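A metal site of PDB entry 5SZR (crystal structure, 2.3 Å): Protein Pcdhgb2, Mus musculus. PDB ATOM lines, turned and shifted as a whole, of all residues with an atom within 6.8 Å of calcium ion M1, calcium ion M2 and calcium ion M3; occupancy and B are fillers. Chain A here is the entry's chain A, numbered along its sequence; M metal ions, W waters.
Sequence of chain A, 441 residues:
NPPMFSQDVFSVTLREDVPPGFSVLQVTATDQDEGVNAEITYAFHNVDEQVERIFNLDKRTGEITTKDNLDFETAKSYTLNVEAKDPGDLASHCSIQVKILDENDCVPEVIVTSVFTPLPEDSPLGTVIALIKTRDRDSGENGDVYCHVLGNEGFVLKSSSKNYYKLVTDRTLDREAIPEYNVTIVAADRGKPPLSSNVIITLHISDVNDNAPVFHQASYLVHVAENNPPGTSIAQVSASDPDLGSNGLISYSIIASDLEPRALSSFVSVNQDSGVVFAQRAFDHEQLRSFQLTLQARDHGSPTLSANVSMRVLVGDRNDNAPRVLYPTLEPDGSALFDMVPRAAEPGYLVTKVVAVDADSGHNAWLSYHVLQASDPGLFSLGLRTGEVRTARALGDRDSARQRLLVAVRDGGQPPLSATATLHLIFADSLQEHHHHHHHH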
ATOM      1  N   GLU A  16       4.219  -4.151 -37.400  1.00  0.00           N
ATOM      2  CA  GLU A  16       5.610  -3.713 -37.397  1.00  0.00           C
ATOM      3  C   GLU A  16       6.609  -4.858 -37.565  1.00  0.00           C
ATOM      4  O   GLU A  16       7.787  -4.593 -37.813  1.00  0.00           O
ATOM      5  CB  GLU A  16       5.930  -2.933 -36.124  1.00  0.00           C
ATOM      6  CG  GLU A  16       5.736  -3.710 -34.829  1.00  0.00           C
ATOM      7  CD  GLU A  16       6.384  -3.019 -33.641  1.00  0.00           C
ATOM      8  OE1 GLU A  16       7.393  -2.301 -33.832  1.00  0.00           O
ATOM      9  OE2 GLU A  16       5.886  -3.175 -32.514  1.00  0.00           O
ATOM     10  N   LEU A  70      10.389  -2.694 -40.212  1.00  0.00           N
ATOM     11  CA  LEU A  70       9.575  -1.652 -39.619  1.00  0.00           C
ATOM     12  C   LEU A  70       9.846  -1.551 -38.121  1.00  0.00           C
ATOM     13  O   LEU A  70      10.568  -2.370 -37.537  1.00  0.00           O
ATOM     14  CB  LEU A  70       8.094  -1.909 -39.893  1.00  0.00           C
ATOM     15  CG  LEU A  70       7.712  -2.050 -41.379  1.00  0.00           C
ATOM     16  CD1 LEU A  70       6.211  -2.239 -41.575  1.00  0.00           C
ATOM     17  CD2 LEU A  70       8.210  -0.856 -42.174  1.00  0.00           C
ATOM     18  N   ASP A  71       9.284  -0.516 -37.501  1.00  0.00           N
ATOM     19  CA  ASP A  71       9.410  -0.307 -36.067  1.00  0.00           C
ATOM     20  C   ASP A  71       8.394   0.744 -35.612  1.00  0.00           C
ATOM     21  O   ASP A  71       8.573   1.938 -35.874  1.00  0.00           O
ATOM     22  CB  ASP A  71      10.834   0.132 -35.688  1.00  0.00           C
ATOM     23  CG  ASP A  71      11.007   0.385 -34.205  1.00  0.00           C
ATOM     24  OD1 ASP A  71      10.188  -0.107 -33.406  1.00  0.00           O
ATOM     25  OD2 ASP A  71      11.985   1.068 -33.837  1.00  0.00           O
ATOM     26  N   PHE A  72       7.316   0.292 -34.960  1.00  0.00           N
ATOM     27  CA  PHE A  72       6.261   1.201 -34.514  1.00  0.00           C
ATOM     28  C   PHE A  72       6.804   2.254 -33.563  1.00  0.00           C
ATOM     29  O   PHE A  72       6.305   3.379 -33.537  1.00  0.00           O
ATOM     30  CB  PHE A  72       5.148   0.387 -33.846  1.00  0.00           C
ATOM     31  CG  PHE A  72       4.030   1.222 -33.293  1.00  0.00           C
ATOM     32  CD1 PHE A  72       2.959   1.581 -34.090  1.00  0.00           C
ATOM     33  CD2 PHE A  72       4.044   1.645 -31.962  1.00  0.00           C
ATOM     34  CE1 PHE A  72       1.921   2.338 -33.582  1.00  0.00           C
ATOM     35  CE2 PHE A  72       3.007   2.402 -31.455  1.00  0.00           C
ATOM     36  CZ  PHE A  72       1.936   2.755 -32.264  1.00  0.00           C
ATOM     37  N   GLU A  73       7.824   1.910 -32.770  1.00  0.00           N
ATOM     38  CA  GLU A  73       8.373   2.864 -31.825  1.00  0.00           C
ATOM     39  C   GLU A  73       9.128   3.990 -32.522  1.00  0.00           C
ATOM     40  O   GLU A  73       9.317   5.055 -31.923  1.00  0.00           O
ATOM     41  CB  GLU A  73       9.292   2.137 -30.829  1.00  0.00           C
ATOM     42  CG  GLU A  73       8.560   1.372 -29.722  1.00  0.00           C
ATOM     43  CD  GLU A  73       7.627   0.276 -30.245  1.00  0.00           C
ATOM     44  OE1 GLU A  73       8.056  -0.517 -31.103  1.00  0.00           O
ATOM     45  OE2 GLU A  73       6.468   0.222 -29.781  1.00  0.00           O
ATOM     46  N   THR A  74       9.553   3.785 -33.773  1.00  0.00           N
ATOM     47  CA  THR A  74      10.247   4.801 -34.555  1.00  0.00           C
ATOM     48  C   THR A  74       9.320   5.582 -35.481  1.00  0.00           C
ATOM     49  O   THR A  74       9.445   6.796 -35.604  1.00  0.00           O
ATOM     50  CB  THR A  74      11.368   4.151 -35.387  1.00  0.00           C
ATOM     51  OG1 THR A  74      12.250   3.423 -34.532  1.00  0.00           O
ATOM     52  CG2 THR A  74      12.158   5.207 -36.137  1.00  0.00           C
ATOM     53  N   LEU A 101       1.018  -0.994 -37.075  1.00  0.00           N
ATOM     54  CA  LEU A 101       0.392  -1.555 -35.885  1.00  0.00           C
ATOM     55  C   LEU A 101       1.446  -1.915 -34.846  1.00  0.00           C
ATOM     56  O   LEU A 101       2.501  -2.461 -35.183  1.00  0.00           O
ATOM     57  CB  LEU A 101      -0.446  -2.790 -36.237  1.00  0.00           C
ATOM     58  CG  LEU A 101      -1.669  -2.475 -37.092  1.00  0.00           C
ATOM     59  CD1 LEU A 101      -2.413  -3.749 -37.457  1.00  0.00           C
ATOM     60  CD2 LEU A 101      -2.578  -1.499 -36.361  1.00  0.00           C
ATOM     61  N   ASP A 102       1.160  -1.593 -33.589  1.00  0.00           N
ATOM     62  CA  ASP A 102       2.094  -1.846 -32.511  1.00  0.00           C
ATOM     63  C   ASP A 102       2.064  -3.323 -32.108  1.00  0.00           C
ATOM     64  O   ASP A 102       0.996  -3.881 -31.848  1.00  0.00           O
ATOM     65  CB  ASP A 102       1.759  -0.975 -31.300  1.00  0.00           C
ATOM     66  CG  ASP A 102       2.484  -1.401 -30.046  1.00  0.00           C
ATOM     67  OD1 ASP A 102       3.699  -1.676 -30.123  1.00  0.00           O
ATOM     68  OD2 ASP A 102       1.840  -1.473 -28.974  1.00  0.00           O
ATOM     69  N   GLU A 103       3.239  -3.938 -32.070  1.00  0.00           N
ATOM     70  CA  GLU A 103       3.422  -5.275 -31.525  1.00  0.00           C
ATOM     71  C   GLU A 103       4.217  -5.191 -30.228  1.00  0.00           C
ATOM     72  O   GLU A 103       4.957  -4.228 -29.985  1.00  0.00           O
ATOM     73  CB  GLU A 103       4.159  -6.186 -32.521  1.00  0.00           C
ATOM     74  CG  GLU A 103       3.474  -6.337 -33.880  1.00  0.00           C
ATOM     75  CD  GLU A 103       2.181  -7.129 -33.802  1.00  0.00           C
ATOM     76  OE1 GLU A 103       1.201  -6.724 -34.471  1.00  0.00           O
ATOM     77  OE2 GLU A 103       2.147  -8.133 -33.074  1.00  0.00           O
ATOM     78  N   ASN A 104       4.052  -6.219 -29.404  1.00  0.00           N
ATOM     79  CA  ASN A 104       4.745  -6.307 -28.118  1.00  0.00           C
ATOM     80  C   ASN A 104       6.158  -6.823 -28.378  1.00  0.00           C
ATOM     81  O   ASN A 104       6.423  -8.027 -28.328  1.00  0.00           O
ATOM     82  CB  ASN A 104       3.975  -7.208 -27.160  1.00  0.00           C
ATOM     83  CG  ASN A 104       4.516  -7.166 -25.757  1.00  0.00           C
ATOM     84  OD1 ASN A 104       5.351  -6.324 -25.411  1.00  0.00           O
ATOM     85  ND2 ASN A 104       4.042  -8.073 -24.912  1.00  0.00           N
ATOM     86  N   ASP A 105       7.083  -5.912 -28.669  1.00  0.00           N
ATOM     87  CA  ASP A 105       8.465  -6.281 -28.914  1.00  0.00           C
ATOM     88  C   ASP A 105       9.457  -5.515 -28.042  1.00  0.00           C
ATOM     89  O   ASP A 105      10.661  -5.577 -28.303  1.00  0.00           O
ATOM     90  CB  ASP A 105       8.825  -6.102 -30.399  1.00  0.00           C
ATOM     91  CG  ASP A 105       8.642  -4.681 -30.886  1.00  0.00           C
ATOM     92  OD1 ASP A 105       7.960  -3.891 -30.218  1.00  0.00           O
ATOM     93  OD2 ASP A 105       9.182  -4.359 -31.967  1.00  0.00           O
ATOM     94  N   CYS A 106       8.984  -4.805 -27.017  1.00  0.00           N
ATOM     95  CA  CYS A 106       9.849  -4.078 -26.089  1.00  0.00           C
ATOM     96  C   CYS A 106       9.650  -4.620 -24.689  1.00  0.00           C
ATOM     97  O   CYS A 106       8.526  -4.632 -24.169  1.00  0.00           O
ATOM     98  CB  CYS A 106       9.559  -2.575 -26.130  1.00  0.00           C
ATOM     99  SG  CYS A 106      10.111  -1.744 -27.647  1.00  0.00           S
ATOM    100  N   VAL A 107      10.740  -5.079 -24.080  1.00  0.00           N
ATOM    101  CA  VAL A 107      10.692  -5.695 -22.743  1.00  0.00           C
ATOM    102  C   VAL A 107      10.466  -4.597 -21.702  1.00  0.00           C
ATOM    103  O   VAL A 107      10.950  -3.474 -21.883  1.00  0.00           O
ATOM    104  CB  VAL A 107      11.990  -6.465 -22.472  1.00  0.00           C
ATOM    105  CG1 VAL A 107      12.028  -7.033 -21.061  1.00  0.00           C
ATOM    106  CG2 VAL A 107      12.158  -7.580 -23.504  1.00  0.00           C
ATOM    107  N   PRO A 108       9.712  -4.871 -20.631  1.00  0.00           N
ATOM    108  CA  PRO A 108       9.671  -3.908 -19.518  1.00  0.00           C
ATOM    109  C   PRO A 108      11.017  -3.841 -18.808  1.00  0.00           C
ATOM    110  O   PRO A 108      11.720  -4.843 -18.680  1.00  0.00           O
ATOM    111  CB  PRO A 108       8.594  -4.482 -18.581  1.00  0.00           C
ATOM    112  CG  PRO A 108       7.842  -5.487 -19.404  1.00  0.00           C
ATOM    113  CD  PRO A 108       8.797  -6.003 -20.435  1.00  0.00           C
ATOM    114  N   ASP A 136       8.258   1.037 -20.324  1.00  0.00           N
ATOM    115  CA  ASP A 136       7.970   0.084 -21.397  1.00  0.00           C
ATOM    116  C   ASP A 136       7.733   0.880 -22.672  1.00  0.00           C
ATOM    117  O   ASP A 136       6.786   1.674 -22.735  1.00  0.00           O
ATOM    118  CB  ASP A 136       6.761  -0.782 -21.052  1.00  0.00           C
ATOM    119  CG  ASP A 136       6.639  -1.998 -21.966  1.00  0.00           C
ATOM    120  OD1 ASP A 136       6.615  -1.834 -23.209  1.00  0.00           O
ATOM    121  OD2 ASP A 136       6.590  -3.130 -21.434  1.00  0.00           O
ATOM    122  N   ARG A 137       8.574   0.659 -23.677  1.00  0.00           N
ATOM    123  CA  ARG A 137       8.556   1.489 -24.877  1.00  0.00           C
ATOM    124  C   ARG A 137       7.350   1.229 -25.763  1.00  0.00           C
ATOM    125  O   ARG A 137       7.094   2.026 -26.667  1.00  0.00           O
ATOM    126  CB  ARG A 137       9.846   1.258 -25.666  1.00  0.00           C
ATOM    127  CG  ARG A 137      11.126   1.570 -24.884  1.00  0.00           C
ATOM    128  CD  ARG A 137      12.330   1.550 -25.803  1.00  0.00           C
ATOM    129  NE  ARG A 137      12.075   2.328 -27.012  1.00  0.00           N
ATOM    130  CZ  ARG A 137      12.793   2.263 -28.122  1.00  0.00           C
ATOM    131  NH1 ARG A 137      12.476   3.009 -29.172  1.00  0.00           N
ATOM    132  NH2 ARG A 137      13.846   1.448 -28.193  1.00  0.00           N
ATOM    133  N   ASP A 138       6.598   0.151 -25.527  1.00  0.00           N
ATOM    134  CA  ASP A 138       5.410  -0.153 -26.303  1.00  0.00           C
ATOM    135  C   ASP A 138       4.241   0.721 -25.877  1.00  0.00           C
ATOM    136  O   ASP A 138       4.285   1.428 -24.862  1.00  0.00           O
ATOM    137  CB  ASP A 138       5.041  -1.631 -26.169  1.00  0.00           C
ATOM    138  CG  ASP A 138       6.052  -2.554 -26.812  1.00  0.00           C
ATOM    139  OD1 ASP A 138       6.666  -2.136 -27.817  1.00  0.00           O
ATOM    140  OD2 ASP A 138       6.239  -3.690 -26.323  1.00  0.00           O
ATOM    141  N   SER A 139       3.164   0.664 -26.671  1.00  0.00           N
ATOM    142  CA  SER A 139       1.938   1.408 -26.429  1.00  0.00           C
ATOM    143  C   SER A 139       0.850   0.480 -25.896  1.00  0.00           C
ATOM    144  O   SER A 139       0.923  -0.745 -26.016  1.00  0.00           O
ATOM    145  CB  SER A 139       1.441   2.092 -27.709  1.00  0.00           C
ATOM    146  OG  SER A 139       2.378   3.038 -28.188  1.00  0.00           O
ATOM    147  N   GLU A 141      -1.704  -1.872 -24.099  1.00  0.00           N
ATOM    148  CA  GLU A 141      -1.529  -2.993 -23.182  1.00  0.00           C
ATOM    149  C   GLU A 141      -0.108  -3.541 -23.230  1.00  0.00           C
ATOM    150  O   GLU A 141       0.421  -4.006 -22.216  1.00  0.00           O
ATOM    151  CB  GLU A 141      -2.545  -4.092 -23.505  1.00  0.00           C
ATOM    152  CG  GLU A 141      -3.979  -3.704 -23.204  1.00  0.00           C
ATOM    153  CD  GLU A 141      -4.963  -4.838 -23.435  1.00  0.00           C
ATOM    154  OE1 GLU A 141      -4.505  -5.961 -23.764  1.00  0.00           O
ATOM    155  OE2 GLU A 141      -6.178  -4.608 -23.294  1.00  0.00           O
ATOM    156  N   ASN A 142       0.518  -3.503 -24.412  1.00  0.00           N
ATOM    157  CA  ASN A 142       1.888  -3.977 -24.525  1.00  0.00           C
ATOM    158  C   ASN A 142       2.852  -3.167 -23.665  1.00  0.00           C
ATOM    159  O   ASN A 142       3.904  -3.674 -23.263  1.00  0.00           O
ATOM    160  CB  ASN A 142       2.321  -3.957 -25.994  1.00  0.00           C
ATOM    161  CG  ASN A 142       1.423  -4.813 -26.875  1.00  0.00           C
ATOM    162  OD1 ASN A 142       0.490  -5.459 -26.392  1.00  0.00           O
ATOM    163  ND2 ASN A 142       1.701  -4.813 -28.175  1.00  0.00           N
ATOM    164  N   GLY A 143       2.505  -1.918 -23.360  1.00  0.00           N
ATOM    165  CA  GLY A 143       3.293  -1.078 -22.476  1.00  0.00           C
ATOM    166  C   GLY A 143       2.794  -0.971 -21.056  1.00  0.00           C
ATOM    167  O   GLY A 143       3.393  -0.244 -20.253  1.00  0.00           O
ATOM    168  N   ASP A 144       1.718  -1.664 -20.706  1.00  0.00           N
ATOM    169  CA  ASP A 144       1.168  -1.632 -19.361  1.00  0.00           C
ATOM    170  C   ASP A 144       1.889  -2.669 -18.515  1.00  0.00           C
ATOM    171  O   ASP A 144       1.709  -3.879 -18.720  1.00  0.00           O
ATOM    172  CB  ASP A 144      -0.341  -1.896 -19.399  1.00  0.00           C
ATOM    173  CG  ASP A 144      -1.070  -1.222 -18.255  1.00  0.00           C
ATOM    174  OD1 ASP A 144      -0.782  -0.044 -17.966  1.00  0.00           O
ATOM    175  OD2 ASP A 144      -1.957  -1.864 -17.647  1.00  0.00           O
ATOM    176  N   VAL A 145       2.687  -2.207 -17.550  1.00  0.00           N
ATOM    177  CA  VAL A 145       3.545  -3.063 -16.746  1.00  0.00           C
ATOM    178  C   VAL A 145       3.038  -3.088 -15.306  1.00  0.00           C
ATOM    179  O   VAL A 145       2.533  -2.080 -14.791  1.00  0.00           O
ATOM    180  CB  VAL A 145       5.016  -2.601 -16.798  1.00  0.00           C
ATOM    181  CG1 VAL A 145       5.920  -3.578 -16.049  1.00  0.00           C
ATOM    182  CG2 VAL A 145       5.468  -2.437 -18.223  1.00  0.00           C
ATOM    183  N   ASP A 189       4.593  -7.147 -18.819  1.00  0.00           N
ATOM    184  CA  ASP A 189       3.600  -6.369 -19.544  1.00  0.00           C
ATOM    185  C   ASP A 189       2.352  -7.215 -19.815  1.00  0.00           C
ATOM    186  O   ASP A 189       2.361  -8.442 -19.689  1.00  0.00           O
ATOM    187  CB  ASP A 189       4.169  -5.817 -20.865  1.00  0.00           C
ATOM    188  CG  ASP A 189       4.658  -6.911 -21.813  1.00  0.00           C
ATOM    189  OD1 ASP A 189       4.033  -7.986 -21.917  1.00  0.00           O
ATOM    190  OD2 ASP A 189       5.687  -6.677 -22.491  1.00  0.00           O
ATOM    191  N   ARG A 190       1.280  -6.540 -20.194  1.00  0.00           N
ATOM    192  CA  ARG A 190       0.007  -7.217 -20.450  1.00  0.00           C
ATOM    193  C   ARG A 190      -0.300  -7.263 -21.943  1.00  0.00           C
ATOM    194  O   ARG A 190      -1.419  -6.961 -22.371  1.00  0.00           O
ATOM    195  CB  ARG A 190      -1.115  -6.531 -19.671  1.00  0.00           C
ATOM    196  CG  ARG A 190      -0.932  -6.618 -18.160  1.00  0.00           C
ATOM    197  CD  ARG A 190      -2.023  -5.885 -17.405  1.00  0.00           C
ATOM    198  NE  ARG A 190      -1.902  -6.063 -15.964  1.00  0.00           N
ATOM    199  CZ  ARG A 190      -2.745  -6.776 -15.216  1.00  0.00           C
ATOM    200  NH1 ARG A 190      -3.784  -7.382 -15.783  1.00  0.00           N
ATOM    201  NH2 ARG A 190      -2.553  -6.883 -13.911  1.00  0.00           N
ATOM    202  N   GLY A 191       0.690  -7.655 -22.744  1.00  0.00           N
ATOM    203  CA  GLY A 191       0.504  -7.889 -24.158  1.00  0.00           C
ATOM    204  C   GLY A 191       0.363  -9.370 -24.458  1.00  0.00           C
ATOM    205  O   GLY A 191       0.379 -10.237 -23.589  1.00  0.00           O
ATOM    206  N   LEU A 195       5.735 -10.078 -22.123  1.00  0.00           N
ATOM    207  CA  LEU A 195       7.167 -10.041 -21.874  1.00  0.00           C
ATOM    208  C   LEU A 195       7.427  -9.599 -20.450  1.00  0.00           C
ATOM    209  O   LEU A 195       6.673  -8.811 -19.881  1.00  0.00           O
ATOM    210  CB  LEU A 195       7.869  -9.095 -22.857  1.00  0.00           C
ATOM    211  CG  LEU A 195       7.766  -9.445 -24.347  1.00  0.00           C
ATOM    212  CD1 LEU A 195       8.352  -8.341 -25.205  1.00  0.00           C
ATOM    213  CD2 LEU A 195       8.464 -10.765 -24.620  1.00  0.00           C
HETATM  214 CA    CA M   1       6.285  -2.166 -30.277  1.00  0.00          CA
HETATM  215 CA    CA M   2       9.406  -2.039 -32.294  1.00  0.00          CA
HETATM  216 CA    CA M   3       6.096  -4.473 -23.884  1.00  0.00          CA
HETATM  217  O   HOH W   1      11.630  -1.700 -30.728  1.00  0.00           O
HETATM  218  O   HOH W   2      10.779  -3.141 -33.800  1.00  0.00           O
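Within 4 Å of calcium ion M3: Asn 104, Cys 106, Asp 136, Asp 138, Asn 142 and Asp 189. The nearest printed residue that does not touch calcium ion M3 is Gly 143 (4.4 Å).
Calcium ion M2 is bound by water W2 (2.3 Å), OD2 of Asp 105 (2.4 Å), OE1 of Glu 73 (2.4 Å), OD1 of Asp 71 (2.4 Å), OE1 of Glu 16 (2.5 Å) and water W1 (2.7 Å). Slightly farther from calcium ion M2 lies OD1 of Asp 105 (3.1 Å).
Along chain A the residues within 4 Å of calcium ion M2 span positions 16 to 105.
Calcium ion M1 is bound by the side-chain carboxylate (OD1) of Asp 105 (2.4 Å), the side-chain carboxylate (OE2) of Glu 73 (2.4 Å), the backbone carbonyl oxygen (O) of Glu 103 (2.5 Å), the side-chain carboxylate (OE2) of Glu 16 (2.5 Å), the side-chain carboxylate (OD1) of Asp 138 (2.5 Å), the side-chain carboxylate (OE1) of Glu 73 (2.6 Å) and the side-chain carboxylate (OD1) of Asp 102 (2.6 Å). Calcium ion M1 has seven donor atoms within binding distance.
Of the 27 residues printed, 6 come within 4 Å of calcium ion M1.
The backbone NH of Glu 16 lies within hydrogen-bond range of the backbone carbonyl oxygen of Leu 101, 3.3 Å away. The backbone NH (N) of Phe 72 sits close to the side-chain carboxylate (OE1) of Glu 16 (2.8 Å). The backbone NH (N) of Gly 191 sits close to the side-chain carboxylate (OD1) of Asp 189, at 3.5 Å. OD2 of Asp 71 is in hydrogen-bond range of OG1 of Thr 74. The side-chain amide nitrogen of Asn 142 lies within hydrogen-bond range of the side-chain carboxylate of Asp 102 (3.4 Å). The side-chain carboxylate (OD2) of Asp 102 lies within hydrogen-bond range of the backbone NH (N) of Ser 139 (3.4 Å). The side-chain carboxylate (OD1) of Asp 189 lies within hydrogen-bond range of the backbone NH (N) of Leu 195, 2.7 Å away.
Calcium ion M3 is bound by O of Asn 142, 2.4 Å away. Calcium ion M3 is bound by O of Cys 106, 2.5 Å away. Calcium ion M3 is bound by the side-chain amide oxygen (OD1) of Asn 104, 2.5 Å away. Calcium ion M3 is bound by OD2 of Asp 138 (2.6 Å). Calcium ion M3 is bound by OD2 of Asp 189, at 2.6 Å. Calcium ion M3 is bound by OD1 of Asp 136 (2.8 Å). OD2 of Asp 136 binds calcium ion M3 (2.8 Å).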
